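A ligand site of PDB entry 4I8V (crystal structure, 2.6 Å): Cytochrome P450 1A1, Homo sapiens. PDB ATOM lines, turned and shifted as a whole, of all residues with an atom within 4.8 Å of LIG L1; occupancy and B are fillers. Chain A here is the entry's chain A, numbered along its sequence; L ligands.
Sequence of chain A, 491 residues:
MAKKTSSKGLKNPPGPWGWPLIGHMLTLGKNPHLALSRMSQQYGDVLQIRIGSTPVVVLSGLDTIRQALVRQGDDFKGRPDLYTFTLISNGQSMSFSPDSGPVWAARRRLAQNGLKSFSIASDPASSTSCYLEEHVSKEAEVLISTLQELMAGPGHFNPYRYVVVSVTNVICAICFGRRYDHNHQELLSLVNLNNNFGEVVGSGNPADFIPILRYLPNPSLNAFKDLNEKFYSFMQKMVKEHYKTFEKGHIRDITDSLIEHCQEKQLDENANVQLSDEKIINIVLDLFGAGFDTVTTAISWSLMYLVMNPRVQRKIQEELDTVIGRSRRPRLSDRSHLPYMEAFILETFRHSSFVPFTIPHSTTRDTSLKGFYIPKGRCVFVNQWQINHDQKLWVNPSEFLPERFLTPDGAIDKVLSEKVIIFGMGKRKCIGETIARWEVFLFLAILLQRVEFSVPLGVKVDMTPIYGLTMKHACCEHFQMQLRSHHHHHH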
ATOM      1  N   ARG A  79      14.477 -24.306  -4.594  1.00  0.00           N
ATOM      2  CA  ARG A  79      15.611 -24.971  -3.969  1.00  0.00           C
ATOM      3  C   ARG A  79      15.069 -25.898  -2.903  1.00  0.00           C
ATOM      4  O   ARG A  79      14.160 -25.552  -2.184  1.00  0.00           O
ATOM      5  CB  ARG A  79      16.537 -23.996  -3.247  1.00  0.00           C
ATOM      6  CG  ARG A  79      17.165 -22.968  -4.103  1.00  0.00           C
ATOM      7  CD  ARG A  79      18.316 -23.518  -4.914  1.00  0.00           C
ATOM      8  NE  ARG A  79      19.066 -22.474  -5.553  1.00  0.00           N
ATOM      9  CZ  ARG A  79      19.676 -22.566  -6.699  1.00  0.00           C
ATOM     10  NH1 ARG A  79      19.633 -23.645  -7.433  1.00  0.00           N
ATOM     11  NH2 ARG A  79      20.318 -21.558  -7.158  1.00  0.00           N
ATOM     12  N   MET A  94      19.965 -15.590  -0.379  1.00  0.00           N
ATOM     13  CA  MET A  94      19.176 -15.436  -1.608  1.00  0.00           C
ATOM     14  C   MET A  94      19.253 -16.690  -2.516  1.00  0.00           C
ATOM     15  O   MET A  94      18.262 -17.101  -3.107  1.00  0.00           O
ATOM     16  CB  MET A  94      19.712 -14.238  -2.400  1.00  0.00           C
ATOM     17  CG  MET A  94      18.945 -13.977  -3.687  1.00  0.00           C
ATOM     18  SD  MET A  94      19.714 -12.601  -4.566  1.00  0.00           S
ATOM     19  CE  MET A  94      21.428 -13.120  -4.749  1.00  0.00           C
ATOM     20  N   SER A  95      20.453 -17.249  -2.614  1.00  0.00           N
ATOM     21  CA  SER A  95      20.816 -18.217  -3.546  1.00  0.00           C
ATOM     22  C   SER A  95      20.492 -19.630  -3.078  1.00  0.00           C
ATOM     23  O   SER A  95      20.110 -20.476  -3.874  1.00  0.00           O
ATOM     24  CB  SER A  95      22.318 -18.122  -3.779  1.00  0.00           C
ATOM     25  OG  SER A  95      22.668 -16.808  -4.199  1.00  0.00           O
ATOM     26  N   TRP A 104      12.374 -13.655  -3.150  1.00  0.00           N
ATOM     27  CA  TRP A 104      13.523 -14.067  -3.951  1.00  0.00           C
ATOM     28  C   TRP A 104      13.642 -13.273  -5.216  1.00  0.00           C
ATOM     29  O   TRP A 104      14.692 -12.769  -5.560  1.00  0.00           O
ATOM     30  CB  TRP A 104      13.416 -15.546  -4.313  1.00  0.00           C
ATOM     31  CG  TRP A 104      14.433 -15.916  -5.283  1.00  0.00           C
ATOM     32  CD1 TRP A 104      15.767 -16.074  -5.043  1.00  0.00           C
ATOM     33  CD2 TRP A 104      14.230 -16.114  -6.674  1.00  0.00           C
ATOM     34  NE1 TRP A 104      16.410 -16.350  -6.254  1.00  0.00           N
ATOM     35  CE2 TRP A 104      15.478 -16.378  -7.253  1.00  0.00           C
ATOM     36  CE3 TRP A 104      13.109 -16.098  -7.498  1.00  0.00           C
ATOM     37  CZ2 TRP A 104      15.627 -16.636  -8.587  1.00  0.00           C
ATOM     38  CZ3 TRP A 104      13.269 -16.341  -8.873  1.00  0.00           C
ATOM     39  CH2 TRP A 104      14.510 -16.622  -9.382  1.00  0.00           C
ATOM     40  N   ARG A 108      16.769 -10.974  -6.220  1.00  0.00           N
ATOM     41  CA  ARG A 108      17.475 -11.224  -7.465  1.00  0.00           C
ATOM     42  C   ARG A 108      17.634  -9.950  -8.290  1.00  0.00           C
ATOM     43  O   ARG A 108      18.702  -9.683  -8.833  1.00  0.00           O
ATOM     44  CB  ARG A 108      16.763 -12.297  -8.286  1.00  0.00           C
ATOM     45  CG  ARG A 108      17.480 -12.684  -9.572  1.00  0.00           C
ATOM     46  CD  ARG A 108      17.218 -14.131  -9.937  1.00  0.00           C
ATOM     47  NE  ARG A 108      17.653 -14.439 -11.296  1.00  0.00           N
ATOM     48  CZ  ARG A 108      18.654 -15.273 -11.588  1.00  0.00           C
ATOM     49  NH1 ARG A 108      19.314 -15.893 -10.615  1.00  0.00           N
ATOM     50  NH2 ARG A 108      18.980 -15.495 -12.854  1.00  0.00           N
ATOM     51  N   LEU A 115      25.034  -5.287  -9.496  1.00  0.00           N
ATOM     52  CA  LEU A 115      26.136  -5.741 -10.310  1.00  0.00           C
ATOM     53  C   LEU A 115      26.408  -4.887 -11.480  1.00  0.00           C
ATOM     54  O   LEU A 115      27.570  -4.538 -11.745  1.00  0.00           O
ATOM     55  CB  LEU A 115      25.883  -7.139 -10.801  1.00  0.00           C
ATOM     56  CG  LEU A 115      26.183  -8.168  -9.741  1.00  0.00           C
ATOM     57  CD1 LEU A 115      25.879  -9.539 -10.363  1.00  0.00           C
ATOM     58  CD2 LEU A 115      27.657  -8.020  -9.281  1.00  0.00           C
ATOM     59  N   ILE A 171      36.029  -8.228  -6.699  1.00  0.00           N
ATOM     60  CA  ILE A 171      34.632  -8.377  -6.338  1.00  0.00           C
ATOM     61  C   ILE A 171      34.491  -7.675  -5.006  1.00  0.00           C
ATOM     62  O   ILE A 171      33.409  -7.196  -4.668  1.00  0.00           O
ATOM     63  CB  ILE A 171      34.143  -9.871  -6.317  1.00  0.00           C
ATOM     64  CG1 ILE A 171      32.700  -9.986  -5.837  1.00  0.00           C
ATOM     65  CG2 ILE A 171      34.898 -10.707  -5.297  1.00  0.00           C
ATOM     66  CD1 ILE A 171      31.729  -9.280  -6.729  1.00  0.00           C
ATOM     67  N   ASP A 286      26.229 -13.108  -0.873  1.00  0.00           N
ATOM     68  CA  ASP A 286      26.025 -14.124  -1.902  1.00  0.00           C
ATOM     69  C   ASP A 286      26.835 -13.698  -3.108  1.00  0.00           C
ATOM     70  O   ASP A 286      27.545 -14.499  -3.736  1.00  0.00           O
ATOM     71  CB  ASP A 286      24.527 -14.246  -2.226  1.00  0.00           C
ATOM     72  CG  ASP A 286      23.723 -15.192  -1.243  1.00  0.00           C
ATOM     73  OD1 ASP A 286      22.846 -15.929  -1.788  1.00  0.00           O
ATOM     74  OD2 ASP A 286      23.893 -15.204   0.033  1.00  0.00           O
ATOM     75  N   LEU A 287      26.807 -12.419  -3.446  1.00  0.00           N
ATOM     76  CA  LEU A 287      27.684 -11.929  -4.562  1.00  0.00           C
ATOM     77  C   LEU A 287      29.197 -12.121  -4.300  1.00  0.00           C
ATOM     78  O   LEU A 287      29.936 -12.647  -5.109  1.00  0.00           O
ATOM     79  CB  LEU A 287      27.389 -10.506  -4.846  1.00  0.00           C
ATOM     80  CG  LEU A 287      26.275 -10.094  -5.822  1.00  0.00           C
ATOM     81  CD1 LEU A 287      25.249 -11.161  -6.089  1.00  0.00           C
ATOM     82  CD2 LEU A 287      25.605  -8.833  -5.300  1.00  0.00           C
ATOM     83  N   ALA A 290      30.097 -15.990  -4.161  1.00  0.00           N
ATOM     84  CA  ALA A 290      30.113 -16.556  -5.494  1.00  0.00           C
ATOM     85  C   ALA A 290      31.248 -15.967  -6.348  1.00  0.00           C
ATOM     86  O   ALA A 290      31.886 -16.679  -7.147  1.00  0.00           O
ATOM     87  CB  ALA A 290      28.776 -16.290  -6.164  1.00  0.00           C
ATOM     88  N   GLY A 291      31.510 -14.662  -6.172  1.00  0.00           N
ATOM     89  CA  GLY A 291      32.395 -13.931  -7.052  1.00  0.00           C
ATOM     90  C   GLY A 291      33.840 -14.283  -6.826  1.00  0.00           C
ATOM     91  O   GLY A 291      34.560 -14.583  -7.762  1.00  0.00           O
ATOM     92  N   THR A 294      34.357 -18.758  -7.539  1.00  0.00           N
ATOM     93  CA  THR A 294      34.238 -19.407  -8.809  1.00  0.00           C
ATOM     94  C   THR A 294      35.223 -18.851  -9.801  1.00  0.00           C
ATOM     95  O   THR A 294      35.630 -19.551 -10.742  1.00  0.00           O
ATOM     96  CB  THR A 294      32.824 -19.210  -9.416  1.00  0.00           C
ATOM     97  OG1 THR A 294      32.646 -17.818  -9.716  1.00  0.00           O
ATOM     98  CG2 THR A 294      31.808 -19.660  -8.462  1.00  0.00           C
ATOM     99  N   VAL A 295      35.520 -17.576  -9.671  1.00  0.00           N
ATOM    100  CA  VAL A 295      36.385 -16.964 -10.628  1.00  0.00           C
ATOM    101  C   VAL A 295      37.805 -17.300 -10.271  1.00  0.00           C
ATOM    102  O   VAL A 295      38.587 -17.587 -11.177  1.00  0.00           O
ATOM    103  CB  VAL A 295      36.183 -15.458 -10.687  1.00  0.00           C
ATOM    104  CG1 VAL A 295      37.350 -14.776 -11.406  1.00  0.00           C
ATOM    105  CG2 VAL A 295      34.865 -15.157 -11.399  1.00  0.00           C
ATOM    106  N   ALA A 298      38.215 -20.741 -11.606  1.00  0.00           N
ATOM    107  CA  ALA A 298      38.375 -20.765 -13.067  1.00  0.00           C
ATOM    108  C   ALA A 298      39.798 -20.388 -13.544  1.00  0.00           C
ATOM    109  O   ALA A 298      40.333 -21.041 -14.402  1.00  0.00           O
ATOM    110  CB  ALA A 298      37.360 -19.859 -13.711  1.00  0.00           C
ATOM    111  N   PHE A 349      36.367 -24.292 -19.500  1.00  0.00           N
ATOM    112  CA  PHE A 349      35.062 -24.441 -18.871  1.00  0.00           C
ATOM    113  C   PHE A 349      34.583 -25.843 -19.166  1.00  0.00           C
ATOM    114  O   PHE A 349      34.232 -26.576 -18.246  1.00  0.00           O
ATOM    115  CB  PHE A 349      34.048 -23.385 -19.377  1.00  0.00           C
ATOM    116  CG  PHE A 349      34.262 -21.980 -18.809  1.00  0.00           C
ATOM    117  CD1 PHE A 349      33.627 -20.873 -19.407  1.00  0.00           C
ATOM    118  CD2 PHE A 349      35.067 -21.746 -17.714  1.00  0.00           C
ATOM    119  CE1 PHE A 349      33.815 -19.574 -18.919  1.00  0.00           C
ATOM    120  CE2 PHE A 349      35.240 -20.431 -17.234  1.00  0.00           C
ATOM    121  CZ  PHE A 349      34.617 -19.373 -17.821  1.00  0.00           C
ATOM    122  N   PHE A 354      34.168 -27.376 -13.886  1.00  0.00           N
ATOM    123  CA  PHE A 354      34.504 -27.230 -12.491  1.00  0.00           C
ATOM    124  C   PHE A 354      33.317 -26.851 -11.624  1.00  0.00           C
ATOM    125  O   PHE A 354      33.426 -26.905 -10.413  1.00  0.00           O
ATOM    126  CB  PHE A 354      35.647 -26.239 -12.266  1.00  0.00           C
ATOM    127  CG  PHE A 354      35.266 -24.817 -12.488  1.00  0.00           C
ATOM    128  CD1 PHE A 354      34.875 -24.021 -11.440  1.00  0.00           C
ATOM    129  CD2 PHE A 354      35.271 -24.281 -13.750  1.00  0.00           C
ATOM    130  CE1 PHE A 354      34.522 -22.719 -11.645  1.00  0.00           C
ATOM    131  CE2 PHE A 354      34.914 -22.962 -13.940  1.00  0.00           C
ATOM    132  CZ  PHE A 354      34.529 -22.179 -12.889  1.00  0.00           C
ATOM    133  N   VAL A 355      32.222 -26.422 -12.242  1.00  0.00           N
ATOM    134  CA  VAL A 355      30.938 -26.459 -11.576  1.00  0.00           C
ATOM    135  C   VAL A 355      30.131 -27.612 -12.191  1.00  0.00           C
ATOM    136  O   VAL A 355      29.301 -27.362 -13.023  1.00  0.00           O
ATOM    137  CB  VAL A 355      30.179 -25.132 -11.787  1.00  0.00           C
ATOM    138  CG1 VAL A 355      28.964 -24.999 -10.865  1.00  0.00           C
ATOM    139  CG2 VAL A 355      31.122 -23.990 -11.489  1.00  0.00           C
ATOM    140  N   THR A 358      24.531 -27.715 -11.277  1.00  0.00           N
ATOM    141  CA  THR A 358      24.022 -26.484 -10.706  1.00  0.00           C
ATOM    142  C   THR A 358      23.847 -26.702  -9.205  1.00  0.00           C
ATOM    143  O   THR A 358      23.938 -27.842  -8.693  1.00  0.00           O
ATOM    144  CB  THR A 358      22.642 -26.083 -11.240  1.00  0.00           C
ATOM    145  OG1 THR A 358      21.701 -27.068 -10.844  1.00  0.00           O
ATOM    146  CG2 THR A 358      22.642 -25.965 -12.757  1.00  0.00           C
ATOM    147  N   ILE A 359      23.571 -25.621  -8.503  1.00  0.00           N
ATOM    148  CA  ILE A 359      23.073 -25.734  -7.182  1.00  0.00           C
ATOM    149  C   ILE A 359      21.777 -26.493  -7.419  1.00  0.00           C
ATOM    150  O   ILE A 359      21.075 -26.265  -8.403  1.00  0.00           O
ATOM    151  CB  ILE A 359      22.780 -24.358  -6.587  1.00  0.00           C
ATOM    152  CG1 ILE A 359      24.056 -23.623  -6.388  1.00  0.00           C
ATOM    153  CG2 ILE A 359      22.063 -24.453  -5.261  1.00  0.00           C
ATOM    154  CD1 ILE A 359      23.816 -22.149  -6.165  1.00  0.00           C
ATOM    155  N   HIS A 361      18.069 -27.851  -7.539  1.00  0.00           N
ATOM    156  CA  HIS A 361      16.791 -27.245  -7.752  1.00  0.00           C
ATOM    157  C   HIS A 361      15.749 -28.040  -7.037  1.00  0.00           C
ATOM    158  O   HIS A 361      16.079 -29.000  -6.351  1.00  0.00           O
ATOM    159  CB  HIS A 361      16.468 -27.152  -9.204  1.00  0.00           C
ATOM    160  CG  HIS A 361      17.270 -26.127  -9.923  1.00  0.00           C
ATOM    161  ND1 HIS A 361      16.715 -25.236 -10.824  1.00  0.00           N
ATOM    162  CD2 HIS A 361      18.588 -25.850  -9.872  1.00  0.00           C
ATOM    163  CE1 HIS A 361      17.670 -24.457 -11.306  1.00  0.00           C
ATOM    164  NE2 HIS A 361      18.814 -24.814 -10.748  1.00  0.00           N
ATOM    165  N   GLN A 384      25.554 -30.658 -15.451  1.00  0.00           N
ATOM    166  CA  GLN A 384      26.207 -29.939 -16.521  1.00  0.00           C
ATOM    167  C   GLN A 384      27.442 -30.675 -17.056  1.00  0.00           C
ATOM    168  O   GLN A 384      27.752 -30.612 -18.242  1.00  0.00           O
ATOM    169  CB  GLN A 384      26.667 -28.563 -16.020  1.00  0.00           C
ATOM    170  CG  GLN A 384      25.559 -27.653 -15.555  1.00  0.00           C
ATOM    171  CD  GLN A 384      26.019 -26.220 -15.253  1.00  0.00           C
ATOM    172  OE1 GLN A 384      25.414 -25.266 -15.693  1.00  0.00           O
ATOM    173  NE2 GLN A 384      27.079 -26.072 -14.516  1.00  0.00           N
ATOM    174  N   ILE A 422      28.081 -24.200 -18.292  1.00  0.00           N
ATOM    175  CA  ILE A 422      28.631 -24.080 -16.988  1.00  0.00           C
ATOM    176  C   ILE A 422      28.002 -22.981 -16.100  1.00  0.00           C
ATOM    177  O   ILE A 422      28.254 -22.946 -14.888  1.00  0.00           O
ATOM    178  CB  ILE A 422      30.167 -23.897 -17.127  1.00  0.00           C
ATOM    179  CG1 ILE A 422      30.844 -24.172 -15.799  1.00  0.00           C
ATOM    180  CG2 ILE A 422      30.547 -22.518 -17.638  1.00  0.00           C
ATOM    181  CD1 ILE A 422      32.319 -24.387 -15.927  1.00  0.00           C
ATOM    182  N   PHE A 423      27.113 -22.149 -16.656  1.00  0.00           N
ATOM    183  CA  PHE A 423      26.443 -21.068 -15.847  1.00  0.00           C
ATOM    184  C   PHE A 423      24.955 -21.295 -15.532  1.00  0.00           C
ATOM    185  O   PHE A 423      24.262 -20.361 -15.082  1.00  0.00           O
ATOM    186  CB  PHE A 423      26.590 -19.686 -16.558  1.00  0.00           C
ATOM    187  CG  PHE A 423      27.992 -19.197 -16.657  1.00  0.00           C
ATOM    188  CD1 PHE A 423      28.562 -18.515 -15.623  1.00  0.00           C
ATOM    189  CD2 PHE A 423      28.742 -19.388 -17.820  1.00  0.00           C
ATOM    190  CE1 PHE A 423      29.863 -18.016 -15.739  1.00  0.00           C
ATOM    191  CE2 PHE A 423      30.041 -18.913 -17.930  1.00  0.00           C
ATOM    192  CZ  PHE A 423      30.593 -18.223 -16.884  1.00  0.00           C
ATOM    193  N   GLY A 424      24.449 -22.495 -15.780  1.00  0.00           N
ATOM    194  CA  GLY A 424      23.027 -22.766 -15.650  1.00  0.00           C
ATOM    195  C   GLY A 424      22.209 -22.171 -16.779  1.00  0.00           C
ATOM    196  O   GLY A 424      22.723 -21.855 -17.826  1.00  0.00           O
ATOM    197  N   LYS A 427      15.586 -19.425 -14.847  1.00  0.00           N
ATOM    198  CA  LYS A 427      15.306 -18.507 -13.789  1.00  0.00           C
ATOM    199  C   LYS A 427      16.458 -18.424 -12.788  1.00  0.00           C
ATOM    200  O   LYS A 427      16.706 -17.355 -12.233  1.00  0.00           O
ATOM    201  CB  LYS A 427      14.036 -18.925 -13.098  1.00  0.00           C
ATOM    202  CG  LYS A 427      12.782 -18.721 -13.970  1.00  0.00           C
ATOM    203  CD  LYS A 427      12.393 -17.266 -14.055  1.00  0.00           C
ATOM    204  CE  LYS A 427      11.327 -17.017 -15.104  1.00  0.00           C
ATOM    205  NZ  LYS A 427      10.039 -17.671 -14.738  1.00  0.00           N
ATOM    206  N   ARG A 428      17.161 -19.527 -12.603  1.00  0.00           N
ATOM    207  CA  ARG A 428      18.263 -19.548 -11.648  1.00  0.00           C
ATOM    208  C   ARG A 428      19.634 -19.564 -12.321  1.00  0.00           C
ATOM    209  O   ARG A 428      20.557 -20.191 -11.799  1.00  0.00           O
ATOM    210  CB  ARG A 428      18.124 -20.748 -10.718  1.00  0.00           C
ATOM    211  CG  ARG A 428      16.828 -20.780  -9.925  1.00  0.00           C
ATOM    212  CD  ARG A 428      16.736 -19.592  -8.982  1.00  0.00           C
ATOM    213  NE  ARG A 428      16.060 -19.935  -7.731  1.00  0.00           N
ATOM    214  CZ  ARG A 428      16.587 -19.761  -6.526  1.00  0.00           C
ATOM    215  NH1 ARG A 428      17.807 -19.241  -6.396  1.00  0.00           N
ATOM    216  NH2 ARG A 428      15.904 -20.101  -5.443  1.00  0.00           N
ATOM    217  N   LYS A 429      19.787 -18.858 -13.434  1.00  0.00           N
ATOM    218  CA  LYS A 429      21.087 -18.789 -14.104  1.00  0.00           C
ATOM    219  C   LYS A 429      22.046 -17.818 -13.410  1.00  0.00           C
ATOM    220  O   LYS A 429      21.608 -16.789 -12.875  1.00  0.00           O
ATOM    221  CB  LYS A 429      20.916 -18.406 -15.573  1.00  0.00           C
ATOM    222  CG  LYS A 429      20.524 -16.950 -15.795  1.00  0.00           C
ATOM    223  CD  LYS A 429      20.136 -16.698 -17.244  1.00  0.00           C
ATOM    224  CE  LYS A 429      19.656 -17.974 -17.910  1.00  0.00           C
ATOM    225  NZ  LYS A 429      20.125 -18.058 -19.324  1.00  0.00           N
ATOM    226  N   CYS A 430      23.342 -18.121 -13.419  1.00  0.00           N
ATOM    227  CA  CYS A 430      24.329 -17.256 -12.824  1.00  0.00           C
ATOM    228  C   CYS A 430      23.991 -15.824 -13.169  1.00  0.00           C
ATOM    229  O   CYS A 430      23.711 -15.520 -14.323  1.00  0.00           O
ATOM    230  CB  CYS A 430      25.680 -17.535 -13.374  1.00  0.00           C
ATOM    231  SG  CYS A 430      26.963 -16.782 -12.408  1.00  0.00           S
ATOM    232  N   ILE A 431      23.956 -14.953 -12.185  1.00  0.00           N
ATOM    233  CA  ILE A 431      23.826 -13.548 -12.506  1.00  0.00           C
ATOM    234  C   ILE A 431      25.135 -12.838 -12.636  1.00  0.00           C
ATOM    235  O   ILE A 431      25.140 -11.671 -12.977  1.00  0.00           O
ATOM    236  CB  ILE A 431      22.956 -12.798 -11.532  1.00  0.00           C
ATOM    237  CG1 ILE A 431      23.547 -12.793 -10.172  1.00  0.00           C
ATOM    238  CG2 ILE A 431      21.565 -13.395 -11.548  1.00  0.00           C
ATOM    239  CD1 ILE A 431      22.686 -11.979  -9.226  1.00  0.00           C
ATOM    240  N   GLY A 432      26.211 -13.562 -12.360  1.00  0.00           N
ATOM    241  CA  GLY A 432      27.580 -13.087 -12.493  1.00  0.00           C
ATOM    242  C   GLY A 432      28.209 -13.392 -13.845  1.00  0.00           C
ATOM    243  O   GLY A 432      29.377 -13.099 -14.026  1.00  0.00           O
ATOM    244  N   ILE A 435      30.231 -10.690 -15.808  1.00  0.00           N
ATOM    245  CA  ILE A 435      31.434 -10.264 -15.085  1.00  0.00           C
ATOM    246  C   ILE A 435      32.465 -11.349 -15.138  1.00  0.00           C
ATOM    247  O   ILE A 435      33.643 -11.085 -15.385  1.00  0.00           O
ATOM    248  CB  ILE A 435      31.163  -9.958 -13.612  1.00  0.00           C
ATOM    249  CG1 ILE A 435      30.375  -8.700 -13.503  1.00  0.00           C
ATOM    250  CG2 ILE A 435      32.455  -9.843 -12.765  1.00  0.00           C
ATOM    251  CD1 ILE A 435      29.692  -8.606 -12.148  1.00  0.00           C
ATOM    252  N   ALA A 436      32.023 -12.575 -14.880  1.00  0.00           N
ATOM    253  CA  ALA A 436      32.943 -13.724 -14.872  1.00  0.00           C
ATOM    254  C   ALA A 436      33.651 -13.883 -16.210  1.00  0.00           C
ATOM    255  O   ALA A 436      34.864 -13.989 -16.222  1.00  0.00           O
ATOM    256  CB  ALA A 436      32.201 -15.005 -14.510  1.00  0.00           C
HETATM  257  C1  LIG L   1      24.622 -19.168  -9.579  1.00  0.00           C
HETATM  258  C2  LIG L   1      28.265 -20.601 -12.233  1.00  0.00           C
HETATM  259  C3  LIG L   1      30.608 -16.481 -11.360  1.00  0.00           C
HETATM  260  C4  LIG L   1      26.868 -15.002  -8.709  1.00  0.00           C
HETATM  261  C5  LIG L   1      25.429 -19.929 -10.368  1.00  0.00           C
HETATM  262  C6  LIG L   1      25.131 -21.224 -10.828  1.00  0.00           C
HETATM  263  C7  LIG L   1      26.170 -21.617 -11.557  1.00  0.00           C
HETATM  264  C8  LIG L   1      27.069 -20.544 -11.613  1.00  0.00           C
HETATM  265  C9  LIG L   1      26.335 -22.972 -12.215  1.00  0.00           C
HETATM  266  C10 LIG L   1      23.950 -22.106 -10.474  1.00  0.00           C
HETATM  267  C11 LIG L   1      22.674 -21.969 -11.304  1.00  0.00           C
HETATM  268  C12 LIG L   1      21.578 -22.819 -10.707  1.00  0.00           C
HETATM  269  O1  LIG L   1      20.645 -23.167 -11.500  1.00  0.00           O
HETATM  270  O2  LIG L   1      21.521 -23.176  -9.467  1.00  0.00           O
HETATM  271  C13 LIG L   1      29.229 -19.600 -12.187  1.00  0.00           C
HETATM  272  C14 LIG L   1      30.469 -19.758 -12.837  1.00  0.00           C
HETATM  273  C15 LIG L   1      31.141 -18.611 -12.596  1.00  0.00           C
HETATM  274  C16 LIG L   1      30.263 -17.766 -11.750  1.00  0.00           C
HETATM  275  C17 LIG L   1      30.926 -20.923 -13.637  1.00  0.00           C
HETATM  276  C18 LIG L   1      32.456 -18.212 -13.039  1.00  0.00           C
HETATM  277  C19 LIG L   1      33.235 -18.897 -13.817  1.00  0.00           C
HETATM  278  C20 LIG L   1      29.796 -15.670 -10.588  1.00  0.00           C
HETATM  279  C21 LIG L   1      30.128 -14.390 -10.130  1.00  0.00           C
HETATM  280  C22 LIG L   1      29.051 -13.980  -9.376  1.00  0.00           C
HETATM  281  C23 LIG L   1      28.090 -15.021  -9.377  1.00  0.00           C
HETATM  282  C24 LIG L   1      31.383 -13.589 -10.470  1.00  0.00           C
HETATM  283  C25 LIG L   1      28.855 -12.685  -8.692  1.00  0.00           C
HETATM  284  C26 LIG L   1      29.675 -11.671  -8.766  1.00  0.00           C
HETATM  285  C27 LIG L   1      26.001 -16.079  -8.734  1.00  0.00           C
HETATM  286  C28 LIG L   1      24.804 -16.037  -7.944  1.00  0.00           C
HETATM  287  C29 LIG L   1      24.167 -17.170  -8.205  1.00  0.00           C
HETATM  288  C30 LIG L   1      24.991 -17.914  -9.150  1.00  0.00           C
HETATM  289  C31 LIG L   1      24.270 -14.936  -7.040  1.00  0.00           C
HETATM  290  C32 LIG L   1      22.845 -17.585  -7.584  1.00  0.00           C
HETATM  291  C33 LIG L   1      21.645 -17.331  -8.518  1.00  0.00           C
HETATM  292  C34 LIG L   1      20.350 -17.802  -7.876  1.00  0.00           C
HETATM  293  O3  LIG L   1      19.176 -17.480  -8.309  1.00  0.00           O
HETATM  294  O4  LIG L   1      20.494 -18.558  -6.874  1.00  0.00           O
HETATM  295  N1  LIG L   1      26.618 -19.504 -10.911  1.00  0.00           N
HETATM  296  N2  LIG L   1      29.168 -18.412 -11.607  1.00  0.00           N
HETATM  297  N3  LIG L   1      28.579 -16.019 -10.142  1.00  0.00           N
HETATM  298  N4  LIG L   1      26.063 -17.194  -9.522  1.00  0.00           N
HETATM  299 FE1  LIG L   1      27.546 -17.771 -10.568  1.00  0.00          FE
HETATM  300  C1  LG2 L   2      31.129 -19.952  -2.990  1.00  0.00           C
HETATM  301  C2  LG2 L   2      31.730 -19.698  -1.713  1.00  0.00           C
HETATM  302  O1  LG2 L   2      32.914 -20.005  -1.376  1.00  0.00           O
HETATM  303  C3  LG2 L   2      30.896 -19.013  -0.700  1.00  0.00           C
HETATM  304  C4  LG2 L   2      31.378 -18.716   0.567  1.00  0.00           C
HETATM  305  C5  LG2 L   2      30.545 -18.066   1.505  1.00  0.00           C
HETATM  306  C6  LG2 L   2      29.235 -17.704   1.156  1.00  0.00           C
HETATM  307  C7  LG2 L   2      28.361 -17.080   2.010  1.00  0.00           C
HETATM  308  C8  LG2 L   2      27.067 -16.769   1.592  1.00  0.00           C
HETATM  309  C9  LG2 L   2      26.607 -17.041   0.310  1.00  0.00           C
HETATM  310  C10 LG2 L   2      27.418 -17.643  -0.606  1.00  0.00           C
HETATM  311  C11 LG2 L   2      28.689 -17.973  -0.186  1.00  0.00           C
HETATM  312  C12 LG2 L   2      29.543 -18.642  -1.111  1.00  0.00           C
HETATM  313  O2  LG2 L   2      28.992 -18.889  -2.343  1.00  0.00           O
HETATM  314  C13 LG2 L   2      29.776 -19.538  -3.268  1.00  0.00           C
HETATM  315  C14 LG2 L   2      28.992 -19.713  -4.518  1.00  0.00           C
HETATM  316  C15 LG2 L   2      27.732 -19.099  -4.538  1.00  0.00           C
HETATM  317  C16 LG2 L   2      26.931 -19.262  -5.650  1.00  0.00           C
HETATM  318  C17 LG2 L   2      27.421 -19.998  -6.745  1.00  0.00           C
HETATM  319  C18 LG2 L   2      28.679 -20.630  -6.733  1.00  0.00           C
HETATM  320  C19 LG2 L   2      29.482 -20.479  -5.594  1.00  0.00           C
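SG of Cys 430 binds FE1 of LIG L1 (2.2 Å). A ring nitrogen (NE2) of His 361 sits at hydrogen-bond distance from an oxygen (O1) of LIG L1. The guanidinium group of Arg 108 lies within salt-bridge range of an oxygen (O3) of LIG L1 (2.8 Å). O of Arg 428 sits close to O1 of LIG L1 (3.0 Å). O4 of LIG L1 lies within salt-bridge range of NH1 of Arg 428, at 2.8 Å. O2 of LIG L1 lies within salt-bridge range of NH1 of Arg 79, 2.8 Å away. O2 of LIG L1 lies within hydrogen-bond range of N of Ile 359, at 3.3 Å.
The backbone NH (N) of Gly 432 lies close to the side-chain sulfur (SG) of Cys 430, at 3.3 Å. The backbone NH (N) of Arg 108 sits at hydrogen-bond distance from the side-chain sulfur (SD) of Met 94 (3.7 Å). The backbone carbonyl oxygen of Lys 429 sits at hydrogen-bond distance from the guanidinium group of Arg 108. NH1 of Arg 79 sits at hydrogen-bond distance from O of Ile 359 (3.1 Å). The guanidinium group of Arg 79 is in hydrogen-bond range of the backbone carbonyl oxygen of Ser 95, at 2.8 Å. The side-chain carboxylate (OD1) of Asp 286 is in hydrogen-bond range of the side-chain hydroxyl (OG) of Ser 95 (2.6 Å). The backbone carbonyl oxygen of Val 355 is in hydrogen-bond range of the side-chain amide nitrogen of Gln 384 (3.0 Å). The side-chain amide oxygen (OE1) of Gln 384 sits at hydrogen-bond distance from the backbone NH (N) of Gly 424, at 2.9 Å.
Ser 95 touches LIG L1. Trp 104 touches LIG L1 (NE1 to O3, 3.6 Å). Ile 171 touches LIG L1. O of Leu 287 touches C25 of LIG L1 (3.7 Å). Ala 290 touches LIG L1. Gly 291 touches LIG L1 (CA to C24, 3.6 Å). OG1 of Thr 294 touches C3 of LIG L1 (2.9 Å). Val 295 touches LIG L1 (CG2 to C24, 3.9 Å). Phe 354 touches LIG L1 (CZ to C19, 3.6 Å). Val 355 touches LIG L1. Thr 358 touches LIG L1 (CB to C12, 3.5 Å). NE2 of Gln 384 touches C9 of LIG L1 (3.9 Å). Ile 422 touches LIG L1 (O to C9, 3.3 Å). CE1 of Phe 423 touches C14 of LIG L1, at 3.4 Å. Ile 431 touches LIG L1. Gly 432 touches LIG L1 (CA to C22, 3.6 Å). CB of Ala 436 touches C18 of LIG L1 (3.5 Å). Hydrophobic or aromatic side chains that line LIG L1: Trp 104, Ile 171, Ala 290, Val 295, Phe 354, Val 355, Ile 359, His 361, Ile 422, Phe 423, Ile 431 and Ala 436. Of the 32 residues printed, 23 come within 4 Å of LIG L1. The nearest printed residue that does not touch LIG L1 is Gly 424 (4.1 Å).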
